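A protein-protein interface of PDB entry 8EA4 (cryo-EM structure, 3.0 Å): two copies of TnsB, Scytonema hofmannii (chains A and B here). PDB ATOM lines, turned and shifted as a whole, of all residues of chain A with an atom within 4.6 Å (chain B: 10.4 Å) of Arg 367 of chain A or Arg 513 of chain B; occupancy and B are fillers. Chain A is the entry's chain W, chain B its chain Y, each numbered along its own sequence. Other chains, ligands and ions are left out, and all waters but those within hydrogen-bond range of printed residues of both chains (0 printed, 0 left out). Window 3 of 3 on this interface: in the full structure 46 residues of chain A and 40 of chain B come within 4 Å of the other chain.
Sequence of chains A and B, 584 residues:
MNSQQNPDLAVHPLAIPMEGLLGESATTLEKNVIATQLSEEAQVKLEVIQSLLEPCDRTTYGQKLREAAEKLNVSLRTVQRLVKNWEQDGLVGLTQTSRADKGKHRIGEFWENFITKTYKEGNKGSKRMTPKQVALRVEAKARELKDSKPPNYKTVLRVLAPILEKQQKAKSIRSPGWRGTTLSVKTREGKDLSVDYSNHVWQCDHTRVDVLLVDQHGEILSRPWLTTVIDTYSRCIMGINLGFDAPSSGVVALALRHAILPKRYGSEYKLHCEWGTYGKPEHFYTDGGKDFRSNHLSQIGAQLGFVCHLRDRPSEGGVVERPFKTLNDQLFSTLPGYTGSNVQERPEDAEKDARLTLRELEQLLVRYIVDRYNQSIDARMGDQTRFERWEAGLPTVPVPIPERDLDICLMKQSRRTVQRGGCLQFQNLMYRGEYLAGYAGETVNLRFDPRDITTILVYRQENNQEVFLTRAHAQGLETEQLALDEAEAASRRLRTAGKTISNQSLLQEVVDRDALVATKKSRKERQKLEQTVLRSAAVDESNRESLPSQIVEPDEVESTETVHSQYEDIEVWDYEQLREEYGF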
ATOM      1  N   TYR A 269       2.549   1.761  25.212  1.00  0.00           N
ATOM      2  CA  TYR A 269       2.504   1.145  23.884  1.00  0.00           C
ATOM      3  C   TYR A 269       1.488   1.815  22.953  1.00  0.00           C
ATOM      4  O   TYR A 269       1.505   1.569  21.754  1.00  0.00           O
ATOM      5  CB  TYR A 269       2.207  -0.347  24.039  1.00  0.00           C
ATOM      6  CG  TYR A 269       3.407  -1.139  24.503  1.00  0.00           C
ATOM      7  CD1 TYR A 269       3.751  -1.209  25.863  1.00  0.00           C
ATOM      8  CD2 TYR A 269       4.206  -1.787  23.552  1.00  0.00           C
ATOM      9  CE1 TYR A 269       4.881  -1.941  26.271  1.00  0.00           C
ATOM     10  CE2 TYR A 269       5.331  -2.522  23.952  1.00  0.00           C
ATOM     11  CZ  TYR A 269       5.669  -2.606  25.314  1.00  0.00           C
ATOM     12  OH  TYR A 269       6.756  -3.326  25.681  1.00  0.00           O
ATOM     13  N   LYS A 270       0.605   2.675  23.476  1.00  0.00           N
ATOM     14  CA  LYS A 270      -0.396   3.465  22.736  1.00  0.00           C
ATOM     15  C   LYS A 270      -1.359   2.649  21.866  1.00  0.00           C
ATOM     16  O   LYS A 270      -1.927   3.194  20.928  1.00  0.00           O
ATOM     17  CB  LYS A 270       0.286   4.604  21.953  1.00  0.00           C
ATOM     18  CG  LYS A 270       1.161   5.520  22.818  1.00  0.00           C
ATOM     19  CD  LYS A 270       1.735   6.663  21.978  1.00  0.00           C
ATOM     20  CE  LYS A 270       2.636   7.531  22.859  1.00  0.00           C
ATOM     21  NZ  LYS A 270       3.170   8.697  22.119  1.00  0.00           N
ATOM     22  N   LEU A 271      -1.554   1.360  22.147  1.00  0.00           N
ATOM     23  CA  LEU A 271      -2.346   0.470  21.292  1.00  0.00           C
ATOM     24  C   LEU A 271      -3.788   0.963  21.151  1.00  0.00           C
ATOM     25  O   LEU A 271      -4.380   1.446  22.115  1.00  0.00           O
ATOM     26  CB  LEU A 271      -2.370  -0.962  21.847  1.00  0.00           C
ATOM     27  CG  LEU A 271      -1.015  -1.629  22.092  1.00  0.00           C
ATOM     28  CD1 LEU A 271      -1.204  -3.050  22.583  1.00  0.00           C
ATOM     29  CD2 LEU A 271      -0.194  -1.693  20.822  1.00  0.00           C
ATOM     30  N   HIS A 272      -4.438   0.586  20.056  1.00  0.00           N
ATOM     31  CA  HIS A 272      -5.868   0.920  19.876  1.00  0.00           C
ATOM     32  C   HIS A 272      -6.597  -0.406  19.858  1.00  0.00           C
ATOM     33  O   HIS A 272      -7.772  -0.427  20.208  1.00  0.00           O
ATOM     34  CB  HIS A 272      -6.087   1.677  18.579  1.00  0.00           C
ATOM     35  CG  HIS A 272      -7.507   2.082  18.346  1.00  0.00           C
ATOM     36  ND1 HIS A 272      -8.552   1.195  18.306  1.00  0.00           N
ATOM     37  CD2 HIS A 272      -8.026   3.323  18.141  1.00  0.00           C
ATOM     38  CE1 HIS A 272      -9.679   1.862  18.080  1.00  0.00           C
ATOM     39  NE2 HIS A 272      -9.375   3.183  17.973  1.00  0.00           N
ATOM     40  N   GLN A 363       8.377  -1.052  21.634  1.00  0.00           N
ATOM     41  CA  GLN A 363       7.113  -0.269  21.591  1.00  0.00           C
ATOM     42  C   GLN A 363       6.604  -0.239  20.144  1.00  0.00           C
ATOM     43  O   GLN A 363       5.401  -0.495  19.943  1.00  0.00           O
ATOM     44  CB  GLN A 363       7.338   1.145  22.134  1.00  0.00           C
ATOM     45  CG  GLN A 363       7.657   1.178  23.621  1.00  0.00           C
ATOM     46  CD  GLN A 363       7.946   2.576  24.109  1.00  0.00           C
ATOM     47  OE1 GLN A 363       8.355   3.447  23.347  1.00  0.00           O
ATOM     48  NE2 GLN A 363       7.729   2.801  25.395  1.00  0.00           N
ATOM     49  N   LEU A 364       7.483   0.050  19.178  1.00  0.00           N
ATOM     50  CA  LEU A 364       7.114   0.106  17.768  1.00  0.00           C
ATOM     51  C   LEU A 364       6.676  -1.258  17.245  1.00  0.00           C
ATOM     52  O   LEU A 364       5.605  -1.372  16.657  1.00  0.00           O
ATOM     53  CB  LEU A 364       8.289   0.635  16.942  1.00  0.00           C
ATOM     54  CG  LEU A 364       8.651   2.092  17.232  1.00  0.00           C
ATOM     55  CD1 LEU A 364       9.871   2.485  16.425  1.00  0.00           C
ATOM     56  CD2 LEU A 364       7.509   3.009  16.837  1.00  0.00           C
ATOM     57  N   LEU A 365       7.460  -2.303  17.480  1.00  0.00           N
ATOM     58  CA  LEU A 365       7.186  -3.628  16.940  1.00  0.00           C
ATOM     59  C   LEU A 365       5.872  -4.222  17.458  1.00  0.00           C
ATOM     60  O   LEU A 365       5.125  -4.824  16.693  1.00  0.00           O
ATOM     61  CB  LEU A 365       8.390  -4.523  17.241  1.00  0.00           C
ATOM     62  CG  LEU A 365       8.245  -5.967  16.759  1.00  0.00           C
ATOM     63  CD1 LEU A 365       8.081  -6.057  15.253  1.00  0.00           C
ATOM     64  CD2 LEU A 365       9.505  -6.740  17.118  1.00  0.00           C
ATOM     65  N   VAL A 366       5.531  -4.019  18.729  1.00  0.00           N
ATOM     66  CA  VAL A 366       4.253  -4.489  19.262  1.00  0.00           C
ATOM     67  C   VAL A 366       3.077  -3.670  18.750  1.00  0.00           C
ATOM     68  O   VAL A 366       2.061  -4.258  18.405  1.00  0.00           O
ATOM     69  CB  VAL A 366       4.284  -4.525  20.785  1.00  0.00           C
ATOM     70  CG1 VAL A 366       2.914  -4.842  21.372  1.00  0.00           C
ATOM     71  CG2 VAL A 366       5.274  -5.596  21.244  1.00  0.00           C
ATOM     72  N   ARG A 367       3.230  -2.349  18.631  1.00  0.00           N
ATOM     73  CA  ARG A 367       2.140  -1.544  18.016  1.00  0.00           C
ATOM     74  C   ARG A 367       1.884  -2.085  16.606  1.00  0.00           C
ATOM     75  O   ARG A 367       0.708  -2.320  16.272  1.00  0.00           O
ATOM     76  CB  ARG A 367       2.519  -0.058  17.989  1.00  0.00           C
ATOM     77  CG  ARG A 367       1.409   0.854  17.485  1.00  0.00           C
ATOM     78  CD  ARG A 367       1.789   2.320  17.565  1.00  0.00           C
ATOM     79  NE  ARG A 367       0.739   3.194  17.061  1.00  0.00           N
ATOM     80  CZ  ARG A 367      -0.308   3.597  17.772  1.00  0.00           C
ATOM     81  NH1 ARG A 367      -1.425   2.890  17.761  1.00  0.00           N
ATOM     82  NH2 ARG A 367      -0.233   4.703  18.492  1.00  0.00           N
ATOM     83  N   TYR A 368       2.945  -2.279  15.817  1.00  0.00           N
ATOM     84  CA  TYR A 368       2.831  -2.822  14.469  1.00  0.00           C
ATOM     85  C   TYR A 368       2.134  -4.186  14.450  1.00  0.00           C
ATOM     86  O   TYR A 368       1.186  -4.365  13.690  1.00  0.00           O
ATOM     87  CB  TYR A 368       4.214  -2.871  13.817  1.00  0.00           C
ATOM     88  CG  TYR A 368       4.225  -3.540  12.463  1.00  0.00           C
ATOM     89  CD1 TYR A 368       3.798  -2.838  11.324  1.00  0.00           C
ATOM     90  CD2 TYR A 368       4.622  -4.879  12.351  1.00  0.00           C
ATOM     91  CE1 TYR A 368       3.745  -3.488  10.081  1.00  0.00           C
ATOM     92  CE2 TYR A 368       4.550  -5.534  11.112  1.00  0.00           C
ATOM     93  CZ  TYR A 368       4.104  -4.841   9.980  1.00  0.00           C
ATOM     94  OH  TYR A 368       3.982  -5.504   8.806  1.00  0.00           O
ATOM     95  N   ILE A 369       2.530  -5.154  15.278  1.00  0.00           N
ATOM     96  CA  ILE A 369       1.917  -6.493  15.255  1.00  0.00           C
ATOM     97  C   ILE A 369       0.457  -6.478  15.709  1.00  0.00           C
ATOM     98  O   ILE A 369      -0.363  -7.164  15.108  1.00  0.00           O
ATOM     99  CB  ILE A 369       2.768  -7.494  16.042  1.00  0.00           C
ATOM    100  CG1 ILE A 369       4.036  -7.797  15.237  1.00  0.00           C
ATOM    101  CG2 ILE A 369       2.013  -8.795  16.321  1.00  0.00           C
ATOM    102  CD1 ILE A 369       5.102  -8.550  16.005  1.00  0.00           C
ATOM    103  N   VAL A 370       0.092  -5.701  16.722  1.00  0.00           N
ATOM    104  CA  VAL A 370      -1.272  -5.666  17.246  1.00  0.00           C
ATOM    105  C   VAL A 370      -2.211  -4.845  16.388  1.00  0.00           C
ATOM    106  O   VAL A 370      -3.286  -5.327  16.052  1.00  0.00           O
ATOM    107  CB  VAL A 370      -1.289  -5.129  18.675  1.00  0.00           C
ATOM    108  CG1 VAL A 370      -2.719  -4.992  19.191  1.00  0.00           C
ATOM    109  CG2 VAL A 370      -0.538  -6.067  19.610  1.00  0.00           C
ATOM    110  N   ASP A 371      -1.846  -3.609  16.050  1.00  0.00           N
ATOM    111  CA  ASP A 371      -2.722  -2.695  15.313  1.00  0.00           C
ATOM    112  C   ASP A 371      -2.648  -2.863  13.799  1.00  0.00           C
ATOM    113  O   ASP A 371      -3.592  -2.462  13.126  1.00  0.00           O
ATOM    114  CB  ASP A 371      -2.411  -1.232  15.637  1.00  0.00           C
ATOM    115  CG  ASP A 371      -2.633  -0.838  17.094  1.00  0.00           C
ATOM    116  OD1 ASP A 371      -3.702  -1.157  17.657  1.00  0.00           O
ATOM    117  OD2 ASP A 371      -1.774  -0.107  17.636  1.00  0.00           O
ATOM    118  N   ARG A 372      -1.572  -3.436  13.241  1.00  0.00           N
ATOM    119  CA  ARG A 372      -1.419  -3.567  11.789  1.00  0.00           C
ATOM    120  C   ARG A 372      -1.287  -4.998  11.295  1.00  0.00           C
ATOM    121  O   ARG A 372      -2.161  -5.442  10.565  1.00  0.00           O
ATOM    122  CB  ARG A 372      -0.342  -2.601  11.283  1.00  0.00           C
ATOM    123  CG  ARG A 372      -0.178  -2.703   9.769  1.00  0.00           C
ATOM    124  CD  ARG A 372       0.644  -1.568   9.158  1.00  0.00           C
ATOM    125  NE  ARG A 372       0.773  -1.818   7.714  1.00  0.00           N
ATOM    126  CZ  ARG A 372      -0.141  -1.593   6.796  1.00  0.00           C
ATOM    127  NH1 ARG A 372      -1.156  -0.802   6.988  1.00  0.00           N
ATOM    128  NH2 ARG A 372      -0.060  -2.188   5.649  1.00  0.00           N
ATOM    129  N   SER B 505      -9.025   2.362   8.943  1.00  0.00           N
ATOM    130  CA  SER B 505      -8.184   3.399   9.577  1.00  0.00           C
ATOM    131  C   SER B 505      -7.055   2.893  10.482  1.00  0.00           C
ATOM    132  O   SER B 505      -5.943   3.399  10.355  1.00  0.00           O
ATOM    133  CB  SER B 505      -9.055   4.414  10.324  1.00  0.00           C
ATOM    134  OG  SER B 505      -9.758   3.787  11.376  1.00  0.00           O
ATOM    135  N   LEU B 506      -7.253   1.854  11.301  1.00  0.00           N
ATOM    136  CA  LEU B 506      -6.199   1.223  12.111  1.00  0.00           C
ATOM    137  C   LEU B 506      -4.910   0.979  11.312  1.00  0.00           C
ATOM    138  O   LEU B 506      -3.816   1.296  11.765  1.00  0.00           O
ATOM    139  CB  LEU B 506      -6.686  -0.138  12.635  1.00  0.00           C
ATOM    140  CG  LEU B 506      -8.016  -0.165  13.398  1.00  0.00           C
ATOM    141  CD1 LEU B 506      -8.391  -1.611  13.726  1.00  0.00           C
ATOM    142  CD2 LEU B 506      -7.935   0.614  14.698  1.00  0.00           C
ATOM    143  N   LEU B 507      -5.060   0.484  10.082  1.00  0.00           N
ATOM    144  CA  LEU B 507      -3.987   0.119   9.160  1.00  0.00           C
ATOM    145  C   LEU B 507      -3.153   1.318   8.689  1.00  0.00           C
ATOM    146  O   LEU B 507      -2.047   1.121   8.197  1.00  0.00           O
ATOM    147  CB  LEU B 507      -4.610  -0.607   7.943  1.00  0.00           C
ATOM    148  CG  LEU B 507      -5.485  -1.845   8.236  1.00  0.00           C
ATOM    149  CD1 LEU B 507      -6.032  -2.449   6.952  1.00  0.00           C
ATOM    150  CD2 LEU B 507      -4.702  -2.947   8.911  1.00  0.00           C
ATOM    151  N   GLN B 508      -3.670   2.533   8.899  1.00  0.00           N
ATOM    152  CA  GLN B 508      -2.937   3.761   8.492  1.00  0.00           C
ATOM    153  C   GLN B 508      -2.512   4.547   9.735  1.00  0.00           C
ATOM    154  O   GLN B 508      -1.396   5.103   9.726  1.00  0.00           O
ATOM    155  CB  GLN B 508      -3.809   4.617   7.571  1.00  0.00           C
ATOM    156  CG  GLN B 508      -4.125   3.951   6.242  1.00  0.00           C
ATOM    157  CD  GLN B 508      -2.887   3.747   5.407  1.00  0.00           C
ATOM    158  OE1 GLN B 508      -2.326   2.655   5.353  1.00  0.00           O
ATOM    159  NE2 GLN B 508      -2.454   4.801   4.738  1.00  0.00           N
ATOM    160  N   GLU B 509      -3.364   4.599  10.764  1.00  0.00           N
ATOM    161  CA  GLU B 509      -3.046   5.383  11.967  1.00  0.00           C
ATOM    162  C   GLU B 509      -1.657   5.044  12.516  1.00  0.00           C
ATOM    163  O   GLU B 509      -0.945   5.940  12.968  1.00  0.00           O
ATOM    164  CB  GLU B 509      -4.104   5.146  13.060  1.00  0.00           C
ATOM    165  CG  GLU B 509      -5.525   5.645  12.732  1.00  0.00           C
ATOM    166  CD  GLU B 509      -5.765   7.146  12.938  1.00  0.00           C
ATOM    167  OE1 GLU B 509      -4.797   7.936  12.930  1.00  0.00           O
ATOM    168  OE2 GLU B 509      -6.940   7.547  13.084  1.00  0.00           O
ATOM    169  N   VAL B 510      -1.239   3.778  12.439  1.00  0.00           N
ATOM    170  CA  VAL B 510       0.114   3.359  12.822  1.00  0.00           C
ATOM    171  C   VAL B 510       1.185   4.114  12.052  1.00  0.00           C
ATOM    172  O   VAL B 510       2.211   4.448  12.630  1.00  0.00           O
ATOM    173  CB  VAL B 510       0.307   1.841  12.663  1.00  0.00           C
ATOM    174  CG1 VAL B 510       0.049   1.333  11.248  1.00  0.00           C
ATOM    175  CG2 VAL B 510       1.722   1.389  13.022  1.00  0.00           C
ATOM    176  N   VAL B 511       0.961   4.444  10.781  1.00  0.00           N
ATOM    177  CA  VAL B 511       1.999   4.969   9.888  1.00  0.00           C
ATOM    178  C   VAL B 511       2.502   6.335  10.346  1.00  0.00           C
ATOM    179  O   VAL B 511       3.697   6.594  10.282  1.00  0.00           O
ATOM    180  CB  VAL B 511       1.491   5.022   8.446  1.00  0.00           C
ATOM    181  CG1 VAL B 511       2.580   5.486   7.489  1.00  0.00           C
ATOM    182  CG2 VAL B 511       1.043   3.639   7.974  1.00  0.00           C
ATOM    183  N   ASP B 512       1.634   7.181  10.894  1.00  0.00           N
ATOM    184  CA  ASP B 512       2.066   8.437  11.508  1.00  0.00           C
ATOM    185  C   ASP B 512       2.924   8.206  12.743  1.00  0.00           C
ATOM    186  O   ASP B 512       3.975   8.810  12.888  1.00  0.00           O
ATOM    187  CB  ASP B 512       0.864   9.292  11.901  1.00  0.00           C
ATOM    188  CG  ASP B 512       0.140   9.906  10.712  1.00  0.00           C
ATOM    189  OD1 ASP B 512       0.709   9.935   9.601  1.00  0.00           O
ATOM    190  OD2 ASP B 512      -0.990  10.396  10.906  1.00  0.00           O
ATOM    191  N   ARG B 513       2.508   7.333  13.659  1.00  0.00           N
ATOM    192  CA  ARG B 513       3.236   7.158  14.920  1.00  0.00           C
ATOM    193  C   ARG B 513       4.564   6.452  14.669  1.00  0.00           C
ATOM    194  O   ARG B 513       5.573   6.842  15.232  1.00  0.00           O
ATOM    195  CB  ARG B 513       2.369   6.470  15.984  1.00  0.00           C
ATOM    196  CG  ARG B 513       1.222   7.364  16.498  1.00  0.00           C
ATOM    197  CD  ARG B 513       0.009   7.378  15.560  1.00  0.00           C
ATOM    198  NE  ARG B 513      -1.058   8.283  16.003  1.00  0.00           N
ATOM    199  CZ  ARG B 513      -2.148   8.569  15.312  1.00  0.00           C
ATOM    200  NH1 ARG B 513      -2.380   8.030  14.157  1.00  0.00           N
ATOM    201  NH2 ARG B 513      -3.041   9.388  15.765  1.00  0.00           N
ATOM    202  N   ASP B 514       4.594   5.575  13.664  1.00  0.00           N
ATOM    203  CA  ASP B 514       5.900   4.985  13.269  1.00  0.00           C
ATOM    204  C   ASP B 514       6.777   6.125  12.736  1.00  0.00           C
ATOM    205  O   ASP B 514       7.953   6.197  13.148  1.00  0.00           O
ATOM    206  CB  ASP B 514       5.727   3.859  12.246  1.00  0.00           C
ATOM    207  CG  ASP B 514       7.048   3.268  11.781  1.00  0.00           C
ATOM    208  OD1 ASP B 514       7.644   2.491  12.553  1.00  0.00           O
ATOM    209  OD2 ASP B 514       7.469   3.594  10.655  1.00  0.00           O
ATOM    210  N   ALA B 515       6.233   6.988  11.865  1.00  0.00           N
ATOM    211  CA  ALA B 515       6.982   8.144  11.370  1.00  0.00           C
ATOM    212  C   ALA B 515       7.361   9.185  12.445  1.00  0.00           C
ATOM    213  O   ALA B 515       8.189  10.048  12.165  1.00  0.00           O
ATOM    214  CB  ALA B 515       6.167   8.793  10.248  1.00  0.00           C
ATOM    215  N   LEU B 516       6.777   9.132  13.648  1.00  0.00           N
ATOM    216  CA  LEU B 516       6.892  10.175  14.676  1.00  0.00           C
ATOM    217  C   LEU B 516       7.433   9.698  16.035  1.00  0.00           C
ATOM    218  O   LEU B 516       7.643  10.523  16.919  1.00  0.00           O
ATOM    219  CB  LEU B 516       5.547  10.905  14.812  1.00  0.00           C
ATOM    220  CG  LEU B 516       5.107  11.664  13.545  1.00  0.00           C
ATOM    221  CD1 LEU B 516       3.667  12.146  13.710  1.00  0.00           C
ATOM    222  CD2 LEU B 516       5.998  12.874  13.261  1.00  0.00           C
ATOM    223  N   VAL B 517       7.720   8.406  16.216  1.00  0.00           N
ATOM    224  CA  VAL B 517       8.731   7.935  17.186  1.00  0.00           C
ATOM    225  C   VAL B 517      10.117   8.178  16.600  1.00  0.00           C
ATOM    226  O   VAL B 517      10.978   8.748  17.260  1.00  0.00           O
ATOM    227  CB  VAL B 517       8.539   6.453  17.547  1.00  0.00           C
ATOM    228  CG1 VAL B 517       9.686   5.890  18.386  1.00  0.00           C
ATOM    229  CG2 VAL B 517       7.249   6.238  18.338  1.00  0.00           C
ATOM    230  N   ALA B 518      10.315   7.831  15.327  1.00  0.00           N
ATOM    231  CA  ALA B 518      11.345   8.438  14.489  1.00  0.00           C
ATOM    232  C   ALA B 518      11.013   9.930  14.255  1.00  0.00           C
ATOM    233  O   ALA B 518      10.038  10.449  14.790  1.00  0.00           O
ATOM    234  CB  ALA B 518      11.444   7.624  13.197  1.00  0.00           C
ATOM    235  N   THR B 519      11.931  10.632  13.589  1.00  0.00           N
ATOM    236  CA  THR B 519      11.772  12.105  13.464  1.00  0.00           C
ATOM    237  C   THR B 519      12.065  12.708  14.840  1.00  0.00           C
ATOM    238  O   THR B 519      12.997  13.523  14.939  1.00  0.00           O
ATOM    239  CB  THR B 519      10.384  12.501  12.951  1.00  0.00           C
ATOM    240  OG1 THR B 519      10.200  11.905  11.666  1.00  0.00           O
ATOM    241  CG2 THR B 519      10.194  13.999  12.864  1.00  0.00           C
ATOM    242  N   LYS B 520      11.310  12.301  15.862  1.00  0.00           N
ATOM    243  CA  LYS B 520      11.533  12.809  17.239  1.00  0.00           C
ATOM    244  C   LYS B 520      12.918  12.398  17.738  1.00  0.00           C
ATOM    245  O   LYS B 520      13.581  13.238  18.367  1.00  0.00           O
ATOM    246  CB  LYS B 520      10.467  12.261  18.188  1.00  0.00           C
ATOM    247  CG  LYS B 520      10.531  12.786  19.616  1.00  0.00           C
ATOM    248  CD  LYS B 520       9.534  12.126  20.541  1.00  0.00           C
ATOM    249  CE  LYS B 520       9.376  12.848  21.861  1.00  0.00           C
ATOM    250  NZ  LYS B 520      10.655  12.942  22.603  1.00  0.00           N
ATOM    251  N   LYS B 521      13.348  11.165  17.463  1.00  0.00           N
ATOM    252  CA  LYS B 521      14.635  10.698  18.039  1.00  0.00           C
ATOM    253  C   LYS B 521      15.806  11.129  17.160  1.00  0.00           C
ATOM    254  O   LYS B 521      16.401  10.245  16.523  1.00  0.00           O
ATOM    255  CB  LYS B 521      14.620   9.172  18.145  1.00  0.00           C
ATOM    256  CG  LYS B 521      13.551   8.590  19.060  1.00  0.00           C
ATOM    257  CD  LYS B 521      13.643   7.089  19.171  1.00  0.00           C
ATOM    258  CE  LYS B 521      14.853   6.643  19.966  1.00  0.00           C
ATOM    259  NZ  LYS B 521      14.730   7.013  21.396  1.00  0.00           N
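The guanidinium group (NH1) of Arg 372 of chain A is in hydrogen-bond range of the backbone carbonyl oxygen (O) of Leu 507 of chain B.
The backbone carbonyl oxygen (O) of Lys 270 of chain A sits at hydrogen-bond distance from the guanidinium group (NH1) of Arg 367 of chain A, 3.2 Å away. The backbone NH of His 272 of chain A sits at hydrogen-bond distance from the side-chain carboxylate of Asp 371 of chain A (3.1 Å). The side-chain carboxylate (OD2) of Asp 371 of chain A is in salt-bridge range of the guanidinium group (NH1) of Arg 367 of chain A (3.0 Å). OE1 of Glu 509 of chain B is in salt-bridge range of NH1 of Arg 513 of chain B (2.7 Å).
ND1 of His 272 of chain A touches CD2 of Leu 506 of chain B (3.7 Å). Val 517 of chain B touches Leu 364 of chain A (CG2 to CD2, 3.6 Å). CG of Arg 513 of chain B touches NH2 of Arg 367 of chain A, 3.6 Å away. Asp 371 of chain A touches Leu 506 of chain B. Arg 372 of chain A touches Gln 508 of chain B. Val 510 of chain B touches Arg 372 of chain A.
Leu 364 of chain A touches one residue of chain B. Arg 367 of chain A touches just one residue of chain B: Arg 513. Of the printed residues of chain B, Arg 372 of chain A touches Leu 507 (2.4 Å), Gln 508 (3.999 Å) and Val 510 (3.6 Å). Printed residues of chain A within 4 Å of Val 510 of chain B: Arg 372. Of chain A, only Arg 367 comes within 4 Å of Arg 513 of chain B. The nearest printed residue of chain A that does not touch Arg 513 of chain B is Leu 364 of chain A (4.6 Å). The nearest printed residue of chain B that does not touch Arg 372 of chain A is Val 511 of chain B (5.1 Å).
Of the 17 printed residues of chain B, 6 touch a printed residue of chain A. Hydrophobic or aromatic side chains of chain B that line the printed part of chain A: Leu 506, Leu 507, Val 510 and Val 517. Hydrophobic or aromatic side chains of chain A within 4 Å of the printed part of chain B: His 272 and Leu 364. Among the printed residues, no Asp or Glu carboxylate lies within 4 Å of a Lys or Arg side-chain nitrogen of the other chain.
No position is printed for both chains.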
